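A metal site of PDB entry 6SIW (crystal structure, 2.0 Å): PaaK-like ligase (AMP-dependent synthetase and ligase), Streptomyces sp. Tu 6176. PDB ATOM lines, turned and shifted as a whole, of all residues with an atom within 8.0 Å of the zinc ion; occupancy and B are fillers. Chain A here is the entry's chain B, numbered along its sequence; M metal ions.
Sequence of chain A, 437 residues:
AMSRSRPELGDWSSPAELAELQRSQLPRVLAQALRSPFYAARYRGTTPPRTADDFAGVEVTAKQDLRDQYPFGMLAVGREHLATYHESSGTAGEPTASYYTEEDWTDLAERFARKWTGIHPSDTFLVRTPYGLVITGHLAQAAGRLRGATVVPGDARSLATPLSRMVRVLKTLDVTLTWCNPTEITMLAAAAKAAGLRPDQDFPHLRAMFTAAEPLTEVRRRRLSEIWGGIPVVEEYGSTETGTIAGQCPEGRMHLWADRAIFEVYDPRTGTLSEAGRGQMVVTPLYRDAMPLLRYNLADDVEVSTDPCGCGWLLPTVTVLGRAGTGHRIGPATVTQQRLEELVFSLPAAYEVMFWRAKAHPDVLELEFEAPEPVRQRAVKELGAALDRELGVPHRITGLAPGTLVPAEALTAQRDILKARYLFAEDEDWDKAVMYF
SG of Cys 311 is bound to the zinc ion, at 1.8 Å. The zinc ion is bound by SG of Cys 309, at 2.3 Å. A ring nitrogen (NE2) of His 255 is bound to the zinc ion, 2.4 Å away. The zinc ion has three donor atoms within binding distance. Slightly farther from the zinc ion lies the side-chain sulfur (SG) of Cys 249 (2.8 Å).
SG of Cys 311 sits close to N of Trp 313, at 3.6 Å. The side-chain sulfur (SG) of Cys 309 lies close to the guanidinium group (NE) of Arg 253, 3.1 Å away. A ring nitrogen (ND1) of His 255 is in hydrogen-bond range of the backbone carbonyl oxygen (O) of Leu 315, at 2.8 Å. N of His 255 is in hydrogen-bond range of O of Gly 247 (2.8 Å). The side-chain sulfur (SG) of Cys 249 lies close to the backbone NH (N) of Glu 251, 3.2 Å away. The side-chain sulfur (SG) of Cys 249 is in hydrogen-bond range of the backbone carbonyl oxygen (O) of Arg 253, at 3.4 Å. The side-chain sulfur of Cys 249 is in hydrogen-bond range of the backbone NH of Gly 252, at 3.5 Å.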
ATOM      1  N   GLY A 247     -25.289  21.387   2.606  1.00  0.00           N
ATOM      2  CA  GLY A 247     -26.426  21.491   1.680  1.00  0.00           C
ATOM      3  C   GLY A 247     -27.570  20.651   2.167  1.00  0.00           C
ATOM      4  O   GLY A 247     -27.311  19.603   2.791  1.00  0.00           O
ATOM      5  N   GLN A 248     -28.780  21.097   1.841  1.00  0.00           N
ATOM      6  CA  GLN A 248     -30.051  20.469   2.265  1.00  0.00           C
ATOM      7  C   GLN A 248     -30.209  19.095   1.598  1.00  0.00           C
ATOM      8  O   GLN A 248     -29.884  18.955   0.404  1.00  0.00           O
ATOM      9  CB  GLN A 248     -31.207  21.388   1.882  1.00  0.00           C
ATOM     10  CG  GLN A 248     -32.495  21.094   2.618  1.00  0.00           C
ATOM     11  CD  GLN A 248     -33.642  21.864   2.009  1.00  0.00           C
ATOM     12  OE1 GLN A 248     -34.174  21.498   0.957  1.00  0.00           O
ATOM     13  NE2 GLN A 248     -34.006  22.959   2.651  1.00  0.00           N
ATOM     14  N   CYS A 249     -30.745  18.128   2.327  1.00  0.00           N
ATOM     15  CA  CYS A 249     -31.224  16.823   1.801  1.00  0.00           C
ATOM     16  C   CYS A 249     -32.736  16.932   1.587  1.00  0.00           C
ATOM     17  O   CYS A 249     -33.359  17.896   2.001  1.00  0.00           O
ATOM     18  CB  CYS A 249     -30.956  15.772   2.867  1.00  0.00           C
ATOM     19  SG  CYS A 249     -32.078  16.152   4.277  1.00  0.00           S
ATOM     20  N   PRO A 250     -33.398  15.919   0.981  1.00  0.00           N
ATOM     21  CA  PRO A 250     -34.853  15.965   0.816  1.00  0.00           C
ATOM     22  C   PRO A 250     -35.659  16.085   2.117  1.00  0.00           C
ATOM     23  O   PRO A 250     -36.782  16.495   2.033  1.00  0.00           O
ATOM     24  CB  PRO A 250     -35.166  14.662   0.051  1.00  0.00           C
ATOM     25  CG  PRO A 250     -33.859  14.318  -0.639  1.00  0.00           C
ATOM     26  CD  PRO A 250     -32.791  14.741   0.334  1.00  0.00           C
ATOM     27  N   GLU A 251     -35.087  15.750   3.275  1.00  0.00           N
ATOM     28  CA  GLU A 251     -35.814  15.774   4.583  1.00  0.00           C
ATOM     29  C   GLU A 251     -35.703  17.150   5.232  1.00  0.00           C
ATOM     30  O   GLU A 251     -36.303  17.320   6.305  1.00  0.00           O
ATOM     31  CB  GLU A 251     -35.306  14.686   5.540  1.00  0.00           C
ATOM     32  CG  GLU A 251     -35.651  13.274   5.098  1.00  0.00           C
ATOM     33  CD  GLU A 251     -37.097  13.060   4.683  1.00  0.00           C
ATOM     34  OE1 GLU A 251     -37.339  12.505   3.584  1.00  0.00           O
ATOM     35  OE2 GLU A 251     -37.986  13.489   5.448  1.00  0.00           O
ATOM     36  N   GLY A 252     -34.960  18.090   4.642  1.00  0.00           N
ATOM     37  CA  GLY A 252     -34.987  19.511   5.043  1.00  0.00           C
ATOM     38  C   GLY A 252     -33.867  19.873   5.996  1.00  0.00           C
ATOM     39  O   GLY A 252     -33.839  21.039   6.431  1.00  0.00           O
ATOM     40  N   ARG A 253     -32.930  18.955   6.253  1.00  0.00           N
ATOM     41  CA  ARG A 253     -31.702  19.242   7.045  1.00  0.00           C
ATOM     42  C   ARG A 253     -30.519  19.541   6.110  1.00  0.00           C
ATOM     43  O   ARG A 253     -30.470  19.018   4.986  1.00  0.00           O
ATOM     44  CB  ARG A 253     -31.427  18.085   8.010  1.00  0.00           C
ATOM     45  CG  ARG A 253     -32.479  17.975   9.096  1.00  0.00           C
ATOM     46  CD  ARG A 253     -32.109  16.989  10.191  1.00  0.00           C
ATOM     47  NE  ARG A 253     -32.707  15.683   9.948  1.00  0.00           N
ATOM     48  CZ  ARG A 253     -33.898  15.275  10.393  1.00  0.00           C
ATOM     49  NH1 ARG A 253     -34.657  16.067  11.150  1.00  0.00           N
ATOM     50  NH2 ARG A 253     -34.332  14.074  10.081  1.00  0.00           N
ATOM     51  N   MET A 254     -29.604  20.379   6.569  1.00  0.00           N
ATOM     52  CA  MET A 254     -28.312  20.632   5.876  1.00  0.00           C
ATOM     53  C   MET A 254     -27.275  19.613   6.357  1.00  0.00           C
ATOM     54  O   MET A 254     -27.111  19.437   7.585  1.00  0.00           O
ATOM     55  CB  MET A 254     -27.823  22.056   6.127  1.00  0.00           C
ATOM     56  CG  MET A 254     -28.658  23.099   5.390  1.00  0.00           C
ATOM     57  SD  MET A 254     -27.926  24.769   5.466  1.00  0.00           S
ATOM     58  CE  MET A 254     -28.042  25.133   7.224  1.00  0.00           C
ATOM     59  N   HIS A 255     -26.601  18.950   5.420  1.00  0.00           N
ATOM     60  CA  HIS A 255     -25.521  17.985   5.716  1.00  0.00           C
ATOM     61  C   HIS A 255     -24.172  18.646   5.379  1.00  0.00           C
ATOM     62  O   HIS A 255     -24.093  19.268   4.307  1.00  0.00           O
ATOM     63  CB  HIS A 255     -25.748  16.675   4.945  1.00  0.00           C
ATOM     64  CG  HIS A 255     -26.836  15.841   5.540  1.00  0.00           C
ATOM     65  ND1 HIS A 255     -26.568  14.723   6.319  1.00  0.00           N
ATOM     66  CD2 HIS A 255     -28.185  15.951   5.498  1.00  0.00           C
ATOM     67  CE1 HIS A 255     -27.697  14.175   6.719  1.00  0.00           C
ATOM     68  NE2 HIS A 255     -28.703  14.917   6.256  1.00  0.00           N
ATOM     69  N   ASP A 307     -26.238  12.019  14.208  1.00  0.00           N
ATOM     70  CA  ASP A 307     -27.462  11.178  14.250  1.00  0.00           C
ATOM     71  C   ASP A 307     -27.939  10.953  12.818  1.00  0.00           C
ATOM     72  O   ASP A 307     -28.006  11.896  12.033  1.00  0.00           O
ATOM     73  CB  ASP A 307     -28.538  11.763  15.161  1.00  0.00           C
ATOM     74  CG  ASP A 307     -28.204  11.601  16.639  1.00  0.00           C
ATOM     75  OD1 ASP A 307     -27.362  10.743  16.968  1.00  0.00           O
ATOM     76  OD2 ASP A 307     -28.750  12.357  17.450  1.00  0.00           O
ATOM     77  N   PRO A 308     -28.290   9.718  12.424  1.00  0.00           N
ATOM     78  CA  PRO A 308     -28.669   9.456  11.033  1.00  0.00           C
ATOM     79  C   PRO A 308     -29.928  10.245  10.661  1.00  0.00           C
ATOM     80  O   PRO A 308     -30.775  10.441  11.512  1.00  0.00           O
ATOM     81  CB  PRO A 308     -28.872   7.927  10.985  1.00  0.00           C
ATOM     82  CG  PRO A 308     -29.199   7.560  12.426  1.00  0.00           C
ATOM     83  CD  PRO A 308     -28.396   8.520  13.268  1.00  0.00           C
ATOM     84  N   CYS A 309     -30.016  10.719   9.415  1.00  0.00           N
ATOM     85  CA  CYS A 309     -31.179  11.435   8.829  1.00  0.00           C
ATOM     86  C   CYS A 309     -31.979  10.395   8.003  1.00  0.00           C
ATOM     87  O   CYS A 309     -31.378   9.314   7.556  1.00  0.00           O
ATOM     88  CB  CYS A 309     -30.718  12.624   7.989  1.00  0.00           C
ATOM     89  SG  CYS A 309     -31.991  13.880   7.485  1.00  0.00           S
ATOM     90  N   GLY A 310     -33.299  10.653   7.849  1.00  0.00           N
ATOM     91  CA  GLY A 310     -34.200   9.934   6.932  1.00  0.00           C
ATOM     92  C   GLY A 310     -33.700   9.922   5.489  1.00  0.00           C
ATOM     93  O   GLY A 310     -34.143   9.040   4.749  1.00  0.00           O
ATOM     94  N   CYS A 311     -32.839  10.875   5.074  1.00  0.00           N
ATOM     95  CA  CYS A 311     -32.296  10.943   3.682  1.00  0.00           C
ATOM     96  C   CYS A 311     -31.357   9.770   3.390  1.00  0.00           C
ATOM     97  O   CYS A 311     -31.249   9.368   2.201  1.00  0.00           O
ATOM     98  CB  CYS A 311     -31.649  12.290   3.353  1.00  0.00           C
ATOM     99  SG  CYS A 311     -30.129  12.833   4.335  1.00  0.00           S
ATOM    100  N   GLY A 312     -30.732   9.200   4.434  1.00  0.00           N
ATOM    101  CA  GLY A 312     -29.780   8.076   4.316  1.00  0.00           C
ATOM    102  C   GLY A 312     -28.379   8.544   3.965  1.00  0.00           C
ATOM    103  O   GLY A 312     -27.479   7.703   3.914  1.00  0.00           O
ATOM    104  N   TRP A 313     -28.170   9.847   3.733  1.00  0.00           N
ATOM    105  CA  TRP A 313     -26.817  10.423   3.450  1.00  0.00           C
ATOM    106  C   TRP A 313     -25.914  10.163   4.657  1.00  0.00           C
ATOM    107  O   TRP A 313     -26.342  10.448   5.799  1.00  0.00           O
ATOM    108  CB  TRP A 313     -26.895  11.933   3.162  1.00  0.00           C
ATOM    109  CG  TRP A 313     -27.611  12.320   1.903  1.00  0.00           C
ATOM    110  CD1 TRP A 313     -28.286  11.510   1.042  1.00  0.00           C
ATOM    111  CD2 TRP A 313     -27.768  13.650   1.392  1.00  0.00           C
ATOM    112  NE1 TRP A 313     -28.840  12.239   0.038  1.00  0.00           N
ATOM    113  CE2 TRP A 313     -28.551  13.563   0.221  1.00  0.00           C
ATOM    114  CE3 TRP A 313     -27.349  14.919   1.819  1.00  0.00           C
ATOM    115  CZ2 TRP A 313     -28.879  14.681  -0.543  1.00  0.00           C
ATOM    116  CZ3 TRP A 313     -27.668  16.024   1.063  1.00  0.00           C
ATOM    117  CH2 TRP A 313     -28.429  15.899  -0.113  1.00  0.00           C
ATOM    118  N   LEU A 314     -24.698   9.652   4.425  1.00  0.00           N
ATOM    119  CA  LEU A 314     -23.774   9.304   5.531  1.00  0.00           C
ATOM    120  C   LEU A 314     -22.896  10.519   5.832  1.00  0.00           C
ATOM    121  O   LEU A 314     -21.671  10.466   5.638  1.00  0.00           O
ATOM    122  CB  LEU A 314     -22.974   8.052   5.152  1.00  0.00           C
ATOM    123  CG  LEU A 314     -23.797   6.778   4.973  1.00  0.00           C
ATOM    124  CD1 LEU A 314     -22.893   5.638   4.527  1.00  0.00           C
ATOM    125  CD2 LEU A 314     -24.511   6.417   6.262  1.00  0.00           C
ATOM    126  N   LEU A 315     -23.537  11.590   6.294  1.00  0.00           N
ATOM    127  CA  LEU A 315     -22.889  12.884   6.605  1.00  0.00           C
ATOM    128  C   LEU A 315     -23.583  13.490   7.810  1.00  0.00           C
ATOM    129  O   LEU A 315     -24.797  13.390   7.958  1.00  0.00           O
ATOM    130  CB  LEU A 315     -22.986  13.796   5.387  1.00  0.00           C
ATOM    131  CG  LEU A 315     -22.116  13.405   4.191  1.00  0.00           C
ATOM    132  CD1 LEU A 315     -22.562  14.150   2.944  1.00  0.00           C
ATOM    133  CD2 LEU A 315     -20.641  13.634   4.475  1.00  0.00           C
ATOM    134  N   PRO A 316     -22.823  14.157   8.709  1.00  0.00           N
ATOM    135  CA  PRO A 316     -23.425  14.871   9.830  1.00  0.00           C
ATOM    136  C   PRO A 316     -24.306  16.025   9.328  1.00  0.00           C
ATOM    137  O   PRO A 316     -24.094  16.505   8.226  1.00  0.00           O
ATOM    138  CB  PRO A 316     -22.226  15.421  10.630  1.00  0.00           C
ATOM    139  CG  PRO A 316     -21.031  14.605  10.130  1.00  0.00           C
ATOM    140  CD  PRO A 316     -21.357  14.237   8.705  1.00  0.00           C
ATOM    141  N   THR A 317     -25.281  16.412  10.145  1.00  0.00           N
ATOM    142  CA  THR A 317     -26.166  17.561   9.864  1.00  0.00           C
ATOM    143  C   THR A 317     -25.646  18.760  10.665  1.00  0.00           C
ATOM    144  O   THR A 317     -24.875  18.569  11.627  1.00  0.00           O
ATOM    145  CB  THR A 317     -27.632  17.234  10.165  1.00  0.00           C
ATOM    146  OG1 THR A 317     -27.771  17.105  11.577  1.00  0.00           O
ATOM    147  CG2 THR A 317     -28.106  15.993   9.441  1.00  0.00           C
HETATM  148 ZN    ZN M   1     -30.775  14.018   5.585  1.00  0.00          ZN
